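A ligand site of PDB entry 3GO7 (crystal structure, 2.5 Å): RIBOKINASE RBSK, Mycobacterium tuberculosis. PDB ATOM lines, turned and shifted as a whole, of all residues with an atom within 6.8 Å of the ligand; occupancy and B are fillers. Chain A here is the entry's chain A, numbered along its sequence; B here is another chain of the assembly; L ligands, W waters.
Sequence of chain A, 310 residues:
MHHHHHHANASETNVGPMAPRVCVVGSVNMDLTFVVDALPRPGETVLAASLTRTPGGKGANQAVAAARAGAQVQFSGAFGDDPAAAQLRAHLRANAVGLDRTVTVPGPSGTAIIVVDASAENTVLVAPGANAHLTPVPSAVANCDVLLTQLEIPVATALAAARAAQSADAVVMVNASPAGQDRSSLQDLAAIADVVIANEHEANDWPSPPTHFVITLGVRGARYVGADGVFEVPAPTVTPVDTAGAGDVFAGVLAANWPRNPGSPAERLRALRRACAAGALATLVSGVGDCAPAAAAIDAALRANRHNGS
The side-chain carboxylate (OD2) of Asp 248 is in hydrogen-bond range of an oxygen (O1) of the ligand (2.5 Å).
OE2 of Glu 152 is in hydrogen-bond range of O5 of the ligand, 2.6 Å away.
The side-chain carboxylate of Asp 31 lies within hydrogen-bond range of an oxygen (O4) of the ligand (2.7 Å).
ND2 of Asn 29 is in hydrogen-bond range of O4 of the ligand, 2.8 Å away.
N of Gly 57 is in hydrogen-bond range of O3 of the ligand.
The side-chain amide nitrogen (ND2) of Asn 61 sits at hydrogen-bond distance from an oxygen (O3) of the ligand, at 2.9 Å.
The backbone NH (N) of Lys 58 lies within hydrogen-bond range of an oxygen (O5) of the ligand, at 3.2 Å.
The side-chain amino group (NZ) of Lys 58 lies within hydrogen-bond range of an oxygen (O1) of the ligand (3.4 Å).
OD1 of Asp 248 sits at hydrogen-bond distance from NE2 of Gln 62 (2.9 Å).
OE1 of Glu 152 lies within hydrogen-bond range of ND2 of Asn 29 (3.1 Å).
OE1 of Glu 152 lies within hydrogen-bond range of OG of Ser 27.
N of Asp 31 sits at hydrogen-bond distance from O of Thr 54.
The backbone carbonyl oxygen of Asn 29 lies within hydrogen-bond range of the backbone NH of Gly 56 (2.7 Å).
The backbone carbonyl oxygen (O) of Gly 57 sits close to the side-chain amide nitrogen (ND2) of Asn 61, 3.2 Å away.
NZ of Lys 58 is in hydrogen-bond range of OG1 of Thr 45 of chain B (3.3 Å).
The backbone NH of Ala 112 is in hydrogen-bond range of the backbone carbonyl oxygen of Met 30, at 3.0 Å.
Residues that only touch the ligand: Ala 112 (3.4 Å), Val 288 (3.6 Å), Val 124 (3.6 Å), Gly 56 (3.7 Å) and Val 126 (3.7 Å).
Hydrophobic or aromatic side chains that line the ligand: Ala 112, Val 124, Val 126 and Val 288.
The nearest printed residue that does not touch the ligand is Ile 114 (4.4 Å).
Water W2 lies within hydrogen-bond range of O1 of the ligand (2.7 Å), OD2 of Asp 248 (3.0 Å), N of Gly 245 (3.4 Å) and N of Gly 247 (3.5 Å).
Water W1 lies within hydrogen-bond range of the backbone NH (N) of Gly 245 (3.1 Å), an oxygen (O1) of the ligand (3.3 Å) and the side-chain amide oxygen (OD1) of Asn 122 (3.4 Å).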
ATOM      1  N   SER A  27     -24.128 -22.532  21.490  1.00  0.00           N
ATOM      2  CA  SER A  27     -23.073 -21.653  21.033  1.00  0.00           C
ATOM      3  C   SER A  27     -23.264 -20.239  21.505  1.00  0.00           C
ATOM      4  O   SER A  27     -24.403 -19.789  21.690  1.00  0.00           O
ATOM      5  CB  SER A  27     -23.045 -21.635  19.529  1.00  0.00           C
ATOM      6  OG  SER A  27     -24.362 -21.406  19.079  1.00  0.00           O
ATOM      7  N   VAL A  28     -22.143 -19.561  21.723  1.00  0.00           N
ATOM      8  CA  VAL A  28     -22.127 -18.117  22.004  1.00  0.00           C
ATOM      9  C   VAL A  28     -21.155 -17.421  21.036  1.00  0.00           C
ATOM     10  O   VAL A  28     -20.048 -17.914  20.795  1.00  0.00           O
ATOM     11  CB  VAL A  28     -21.782 -17.841  23.508  1.00  0.00           C
ATOM     12  CG1 VAL A  28     -20.425 -18.494  23.889  1.00  0.00           C
ATOM     13  CG2 VAL A  28     -21.810 -16.350  23.786  1.00  0.00           C
ATOM     14  N   ASN A  29     -21.623 -16.316  20.438  1.00  0.00           N
ATOM     15  CA  ASN A  29     -20.907 -15.576  19.365  1.00  0.00           C
ATOM     16  C   ASN A  29     -20.948 -14.086  19.649  1.00  0.00           C
ATOM     17  O   ASN A  29     -21.871 -13.591  20.312  1.00  0.00           O
ATOM     18  CB  ASN A  29     -21.605 -15.746  18.024  1.00  0.00           C
ATOM     19  CG  ASN A  29     -21.727 -17.201  17.568  1.00  0.00           C
ATOM     20  OD1 ASN A  29     -20.798 -18.004  17.704  1.00  0.00           O
ATOM     21  ND2 ASN A  29     -22.876 -17.539  16.970  1.00  0.00           N
ATOM     22  N   MET A  30     -19.965 -13.342  19.140  1.00  0.00           N
ATOM     23  CA  MET A  30     -20.156 -11.897  19.135  1.00  0.00           C
ATOM     24  C   MET A  30     -20.875 -11.567  17.812  1.00  0.00           C
ATOM     25  O   MET A  30     -20.465 -12.028  16.736  1.00  0.00           O
ATOM     26  CB  MET A  30     -18.823 -11.183  19.309  1.00  0.00           C
ATOM     27  CG  MET A  30     -18.929  -9.672  19.409  1.00  0.00           C
ATOM     28  SD  MET A  30     -19.765  -9.150  20.916  1.00  0.00           S
ATOM     29  CE  MET A  30     -18.417  -9.358  22.110  1.00  0.00           C
ATOM     30  N   ASP A  31     -21.961 -10.828  17.897  1.00  0.00           N
ATOM     31  CA  ASP A  31     -22.708 -10.447  16.722  1.00  0.00           C
ATOM     32  C   ASP A  31     -22.290  -9.076  16.174  1.00  0.00           C
ATOM     33  O   ASP A  31     -22.193  -8.099  16.930  1.00  0.00           O
ATOM     34  CB  ASP A  31     -24.209 -10.413  17.032  1.00  0.00           C
ATOM     35  CG  ASP A  31     -24.809 -11.801  17.242  1.00  0.00           C
ATOM     36  OD1 ASP A  31     -24.139 -12.805  16.941  1.00  0.00           O
ATOM     37  OD2 ASP A  31     -25.967 -11.879  17.716  1.00  0.00           O
ATOM     38  N   THR A  54     -22.685  -6.746  19.432  1.00  0.00           N
ATOM     39  CA  THR A  54     -23.425  -7.139  20.613  1.00  0.00           C
ATOM     40  C   THR A  54     -23.233  -8.643  20.812  1.00  0.00           C
ATOM     41  O   THR A  54     -23.078  -9.387  19.839  1.00  0.00           O
ATOM     42  CB  THR A  54     -24.962  -6.843  20.486  1.00  0.00           C
ATOM     43  OG1 THR A  54     -25.519  -7.525  19.342  1.00  0.00           O
ATOM     44  CG2 THR A  54     -25.267  -5.326  20.382  1.00  0.00           C
ATOM     45  N   PRO A  55     -23.216  -9.090  22.061  1.00  0.00           N
ATOM     46  CA  PRO A  55     -23.199 -10.542  22.341  1.00  0.00           C
ATOM     47  C   PRO A  55     -24.415 -11.320  21.862  1.00  0.00           C
ATOM     48  O   PRO A  55     -25.577 -10.879  21.981  1.00  0.00           O
ATOM     49  CB  PRO A  55     -23.111 -10.604  23.855  1.00  0.00           C
ATOM     50  CG  PRO A  55     -22.420  -9.240  24.211  1.00  0.00           C
ATOM     51  CD  PRO A  55     -23.099  -8.289  23.284  1.00  0.00           C
ATOM     52  N   GLY A  56     -24.158 -12.506  21.346  1.00  0.00           N
ATOM     53  CA  GLY A  56     -25.223 -13.347  20.862  1.00  0.00           C
ATOM     54  C   GLY A  56     -24.829 -14.799  20.764  1.00  0.00           C
ATOM     55  O   GLY A  56     -24.099 -15.293  21.627  1.00  0.00           O
ATOM     56  N   GLY A  57     -25.285 -15.448  19.688  1.00  0.00           N
ATOM     57  CA  GLY A  57     -25.203 -16.906  19.561  1.00  0.00           C
ATOM     58  C   GLY A  57     -26.554 -17.532  19.889  1.00  0.00           C
ATOM     59  O   GLY A  57     -27.217 -17.121  20.857  1.00  0.00           O
ATOM     60  N   LYS A  58     -26.998 -18.480  19.067  1.00  0.00           N
ATOM     61  CA  LYS A  58     -28.226 -19.235  19.339  1.00  0.00           C
ATOM     62  C   LYS A  58     -28.278 -19.751  20.798  1.00  0.00           C
ATOM     63  O   LYS A  58     -29.293 -19.602  21.485  1.00  0.00           O
ATOM     64  CB  LYS A  58     -28.337 -20.411  18.380  1.00  0.00           C
ATOM     65  CG  LYS A  58     -28.608 -20.034  16.951  1.00  0.00           C
ATOM     66  CD  LYS A  58     -28.623 -21.254  16.037  1.00  0.00           C
ATOM     67  CE  LYS A  58     -28.731 -20.823  14.595  1.00  0.00           C
ATOM     68  NZ  LYS A  58     -29.689 -19.660  14.524  1.00  0.00           N
ATOM     69  N   GLY A  59     -27.201 -20.376  21.269  1.00  0.00           N
ATOM     70  CA  GLY A  59     -27.172 -20.937  22.614  1.00  0.00           C
ATOM     71  C   GLY A  59     -27.427 -19.887  23.677  1.00  0.00           C
ATOM     72  O   GLY A  59     -28.297 -20.044  24.533  1.00  0.00           O
ATOM     73  N   ASN A  61     -28.506 -16.598  23.209  1.00  0.00           N
ATOM     74  CA  ASN A  61     -29.807 -15.964  23.042  1.00  0.00           C
ATOM     75  C   ASN A  61     -30.896 -16.822  23.680  1.00  0.00           C
ATOM     76  O   ASN A  61     -31.759 -16.309  24.370  1.00  0.00           O
ATOM     77  CB  ASN A  61     -30.145 -15.736  21.569  1.00  0.00           C
ATOM     78  CG  ASN A  61     -29.138 -14.825  20.850  1.00  0.00           C
ATOM     79  OD1 ASN A  61     -28.372 -14.077  21.484  1.00  0.00           O
ATOM     80  ND2 ASN A  61     -29.148 -14.888  19.518  1.00  0.00           N
ATOM     81  N   GLN A  62     -30.830 -18.133  23.455  1.00  0.00           N
ATOM     82  CA  GLN A  62     -31.870 -19.027  23.957  1.00  0.00           C
ATOM     83  C   GLN A  62     -31.837 -19.176  25.460  1.00  0.00           C
ATOM     84  O   GLN A  62     -32.898 -19.196  26.095  1.00  0.00           O
ATOM     85  CB  GLN A  62     -31.809 -20.390  23.286  1.00  0.00           C
ATOM     86  CG  GLN A  62     -32.354 -20.328  21.899  1.00  0.00           C
ATOM     87  CD  GLN A  62     -32.111 -21.563  21.067  1.00  0.00           C
ATOM     88  OE1 GLN A  62     -31.977 -22.683  21.602  1.00  0.00           O
ATOM     89  NE2 GLN A  62     -32.058 -21.374  19.750  1.00  0.00           N
ATOM     90  N   THR A 111     -18.006 -15.755  15.714  1.00  0.00           N
ATOM     91  CA  THR A 111     -18.423 -14.495  15.144  1.00  0.00           C
ATOM     92  C   THR A 111     -19.640 -14.726  14.286  1.00  0.00           C
ATOM     93  O   THR A 111     -19.685 -15.726  13.587  1.00  0.00           O
ATOM     94  CB  THR A 111     -17.319 -13.893  14.277  1.00  0.00           C
ATOM     95  OG1 THR A 111     -16.093 -13.887  15.010  1.00  0.00           O
ATOM     96  CG2 THR A 111     -17.677 -12.463  13.853  1.00  0.00           C
ATOM     97  N   ALA A 112     -20.595 -13.791  14.309  1.00  0.00           N
ATOM     98  CA  ALA A 112     -21.739 -13.834  13.431  1.00  0.00           C
ATOM     99  C   ALA A 112     -21.972 -12.497  12.764  1.00  0.00           C
ATOM    100  O   ALA A 112     -21.795 -11.433  13.386  1.00  0.00           O
ATOM    101  CB  ALA A 112     -22.993 -14.258  14.170  1.00  0.00           C
ATOM    102  N   ILE A 113     -22.414 -12.569  11.511  1.00  0.00           N
ATOM    103  CA  ILE A 113     -22.810 -11.402  10.791  1.00  0.00           C
ATOM    104  C   ILE A 113     -24.305 -11.545  10.614  1.00  0.00           C
ATOM    105  O   ILE A 113     -24.771 -12.500   9.992  1.00  0.00           O
ATOM    106  CB  ILE A 113     -22.104 -11.329   9.399  1.00  0.00           C
ATOM    107  CG1 ILE A 113     -20.591 -11.563   9.535  1.00  0.00           C
ATOM    108  CG2 ILE A 113     -22.423 -10.041   8.709  1.00  0.00           C
ATOM    109  CD1 ILE A 113     -19.902 -10.675  10.520  1.00  0.00           C
ATOM    110  N   ILE A 114     -25.033 -10.602  11.197  1.00  0.00           N
ATOM    111  CA  ILE A 114     -26.447 -10.462  10.930  1.00  0.00           C
ATOM    112  C   ILE A 114     -26.666  -9.259  10.011  1.00  0.00           C
ATOM    113  O   ILE A 114     -26.102  -8.163  10.213  1.00  0.00           O
ATOM    114  CB  ILE A 114     -27.288 -10.291  12.218  1.00  0.00           C
ATOM    115  CG1 ILE A 114     -27.020 -11.412  13.199  1.00  0.00           C
ATOM    116  CG2 ILE A 114     -28.757 -10.399  11.884  1.00  0.00           C
ATOM    117  CD1 ILE A 114     -25.886 -11.182  14.048  1.00  0.00           C
ATOM    118  N   ASN A 122     -33.856 -10.858   7.712  1.00  0.00           N
ATOM    119  CA  ASN A 122     -32.490 -11.005   8.223  1.00  0.00           C
ATOM    120  C   ASN A 122     -31.799 -12.235   7.658  1.00  0.00           C
ATOM    121  O   ASN A 122     -32.450 -13.238   7.416  1.00  0.00           O
ATOM    122  CB  ASN A 122     -32.481 -11.056   9.756  1.00  0.00           C
ATOM    123  CG  ASN A 122     -32.935 -12.410  10.328  1.00  0.00           C
ATOM    124  OD1 ASN A 122     -32.130 -13.324  10.486  1.00  0.00           O
ATOM    125  ND2 ASN A 122     -34.216 -12.511  10.672  1.00  0.00           N
ATOM    126  N   VAL A 124     -28.192 -14.610   8.514  1.00  0.00           N
ATOM    127  CA  VAL A 124     -27.221 -14.848   9.570  1.00  0.00           C
ATOM    128  C   VAL A 124     -26.092 -15.709   9.015  1.00  0.00           C
ATOM    129  O   VAL A 124     -26.318 -16.757   8.423  1.00  0.00           O
ATOM    130  CB  VAL A 124     -27.874 -15.566  10.826  1.00  0.00           C
ATOM    131  CG1 VAL A 124     -26.828 -16.041  11.812  1.00  0.00           C
ATOM    132  CG2 VAL A 124     -28.919 -14.684  11.495  1.00  0.00           C
ATOM    133  N   LEU A 125     -24.857 -15.265   9.244  1.00  0.00           N
ATOM    134  CA  LEU A 125     -23.691 -15.989   8.851  1.00  0.00           C
ATOM    135  C   LEU A 125     -22.711 -16.122  10.039  1.00  0.00           C
ATOM    136  O   LEU A 125     -22.362 -15.123  10.652  1.00  0.00           O
ATOM    137  CB  LEU A 125     -23.023 -15.206   7.718  1.00  0.00           C
ATOM    138  CG  LEU A 125     -21.651 -15.721   7.304  1.00  0.00           C
ATOM    139  CD1 LEU A 125     -21.843 -17.037   6.585  1.00  0.00           C
ATOM    140  CD2 LEU A 125     -20.933 -14.693   6.421  1.00  0.00           C
ATOM    141  N   VAL A 126     -22.258 -17.330  10.327  1.00  0.00           N
ATOM    142  CA  VAL A 126     -21.515 -17.598  11.544  1.00  0.00           C
ATOM    143  C   VAL A 126     -20.158 -18.238  11.267  1.00  0.00           C
ATOM    144  O   VAL A 126     -20.078 -19.197  10.505  1.00  0.00           O
ATOM    145  CB  VAL A 126     -22.308 -18.567  12.459  1.00  0.00           C
ATOM    146  CG1 VAL A 126     -21.550 -18.850  13.721  1.00  0.00           C
ATOM    147  CG2 VAL A 126     -23.692 -18.018  12.767  1.00  0.00           C
ATOM    148  N   GLU A 152     -24.866 -25.317  15.889  1.00  0.00           N
ATOM    149  CA  GLU A 152     -23.602 -24.598  15.621  1.00  0.00           C
ATOM    150  C   GLU A 152     -22.403 -25.288  16.307  1.00  0.00           C
ATOM    151  O   GLU A 152     -21.240 -25.225  15.843  1.00  0.00           O
ATOM    152  CB  GLU A 152     -23.682 -23.118  16.053  1.00  0.00           C
ATOM    153  CG  GLU A 152     -24.680 -22.302  15.244  1.00  0.00           C
ATOM    154  CD  GLU A 152     -24.742 -20.836  15.646  1.00  0.00           C
ATOM    155  OE1 GLU A 152     -23.968 -20.373  16.524  1.00  0.00           O
ATOM    156  OE2 GLU A 152     -25.595 -20.112  15.064  1.00  0.00           O
ATOM    157  N   ASN A 175     -33.185 -27.225  18.715  1.00  0.00           N
ATOM    158  CA  ASN A 175     -33.428 -26.229  17.653  1.00  0.00           C
ATOM    159  C   ASN A 175     -32.598 -26.673  16.474  1.00  0.00           C
ATOM    160  O   ASN A 175     -31.372 -26.558  16.510  1.00  0.00           O
ATOM    161  CB  ASN A 175     -33.044 -24.812  18.130  1.00  0.00           C
ATOM    162  CG  ASN A 175     -33.127 -23.730  17.019  1.00  0.00           C
ATOM    163  OD1 ASN A 175     -33.997 -23.760  16.125  1.00  0.00           O
ATOM    164  ND2 ASN A 175     -32.228 -22.752  17.104  1.00  0.00           N
ATOM    165  N   ALA A 244     -34.353 -10.646  13.425  1.00  0.00           N
ATOM    166  CA  ALA A 244     -33.164 -11.301  13.929  1.00  0.00           C
ATOM    167  C   ALA A 244     -33.290 -11.561  15.431  1.00  0.00           C
ATOM    168  O   ALA A 244     -33.651 -10.665  16.204  1.00  0.00           O
ATOM    169  CB  ALA A 244     -31.960 -10.467  13.648  1.00  0.00           C
ATOM    170  N   GLY A 245     -33.030 -12.809  15.802  1.00  0.00           N
ATOM    171  CA  GLY A 245     -33.092 -13.218  17.187  1.00  0.00           C
ATOM    172  C   GLY A 245     -34.432 -13.672  17.709  1.00  0.00           C
ATOM    173  O   GLY A 245     -34.492 -14.278  18.777  1.00  0.00           O
ATOM    174  N   ALA A 246     -35.525 -13.382  16.997  1.00  0.00           N
ATOM    175  CA  ALA A 246     -36.875 -13.810  17.434  1.00  0.00           C
ATOM    176  C   ALA A 246     -37.051 -15.320  17.549  1.00  0.00           C
ATOM    177  O   ALA A 246     -37.738 -15.800  18.451  1.00  0.00           O
ATOM    178  CB  ALA A 246     -37.928 -13.232  16.562  1.00  0.00           C
ATOM    179  N   GLY A 247     -36.428 -16.080  16.669  1.00  0.00           N
ATOM    180  CA  GLY A 247     -36.482 -17.532  16.768  1.00  0.00           C
ATOM    181  C   GLY A 247     -35.861 -18.054  18.056  1.00  0.00           C
ATOM    182  O   GLY A 247     -36.454 -18.907  18.747  1.00  0.00           O
ATOM    183  N   ASP A 248     -34.671 -17.536  18.399  1.00  0.00           N
ATOM    184  CA  ASP A 248     -33.985 -17.954  19.641  1.00  0.00           C
ATOM    185  C   ASP A 248     -34.834 -17.648  20.864  1.00  0.00           C
ATOM    186  O   ASP A 248     -34.808 -18.392  21.848  1.00  0.00           O
ATOM    187  CB  ASP A 248     -32.644 -17.261  19.780  1.00  0.00           C
ATOM    188  CG  ASP A 248     -31.660 -17.694  18.727  1.00  0.00           C
ATOM    189  OD1 ASP A 248     -31.704 -18.878  18.320  1.00  0.00           O
ATOM    190  OD2 ASP A 248     -30.834 -16.856  18.295  1.00  0.00           O
ATOM    191  N   VAL A 288     -30.381  -8.451  18.513  1.00  0.00           N
ATOM    192  CA  VAL A 288     -30.503  -9.877  18.406  1.00  0.00           C
ATOM    193  C   VAL A 288     -30.517 -10.472  19.802  1.00  0.00           C
ATOM    194  O   VAL A 288     -31.573 -10.906  20.282  1.00  0.00           O
ATOM    195  CB  VAL A 288     -29.422 -10.440  17.442  1.00  0.00           C
ATOM    196  CG1 VAL A 288     -29.624 -11.921  17.159  1.00  0.00           C
ATOM    197  CG2 VAL A 288     -29.483  -9.689  16.138  1.00  0.00           C
ATOM    198  N   GLY A 289     -29.388 -10.406  20.472  1.00  0.00           N
ATOM    199  CA  GLY A 289     -29.245 -11.060  21.745  1.00  0.00           C
ATOM    200  C   GLY A 289     -29.927 -10.361  22.906  1.00  0.00           C
ATOM    201  O   GLY A 289     -29.976 -10.903  24.006  1.00  0.00           O
ATOM    202  N   THR B  45     -29.628 -19.408   8.546  1.00  0.00           N
ATOM    203  CA  THR B  45     -28.283 -19.383   9.152  1.00  0.00           C
ATOM    204  C   THR B  45     -27.333 -20.293   8.397  1.00  0.00           C
ATOM    205  O   THR B  45     -27.620 -21.464   8.155  1.00  0.00           O
ATOM    206  CB  THR B  45     -28.333 -19.835  10.607  1.00  0.00           C
ATOM    207  OG1 THR B  45     -29.304 -19.057  11.319  1.00  0.00           O
ATOM    208  CG2 THR B  45     -26.939 -19.719  11.279  1.00  0.00           C
HETATM  209  O1  LIG L   1     -30.343 -16.583  15.864  1.00  0.00           O
HETATM  210  C1  LIG L   1     -29.454 -15.455  15.734  1.00  0.00           C
HETATM  211  C2  LIG L   1     -28.061 -15.884  16.233  1.00  0.00           C
HETATM  212  O2  LIG L   1     -27.467 -16.799  15.321  1.00  0.00           O
HETATM  213  C3  LIG L   1     -27.040 -14.777  16.377  1.00  0.00           C
HETATM  214  O3  LIG L   1     -26.997 -14.324  17.730  1.00  0.00           O
HETATM  215  C4  LIG L   1     -25.718 -15.383  15.898  1.00  0.00           C
HETATM  216  O4  LIG L   1     -24.659 -15.404  16.871  1.00  0.00           O
HETATM  217  C5  LIG L   1     -26.047 -16.775  15.394  1.00  0.00           C
HETATM  218  O5  LIG L   1     -25.595 -17.783  16.299  1.00  0.00           O
HETATM  219  O   HOH W   1     -31.880 -14.742  13.605  1.00  0.00           O
HETATM  220  O   HOH W   2     -32.966 -16.159  16.239  1.00  0.00           O
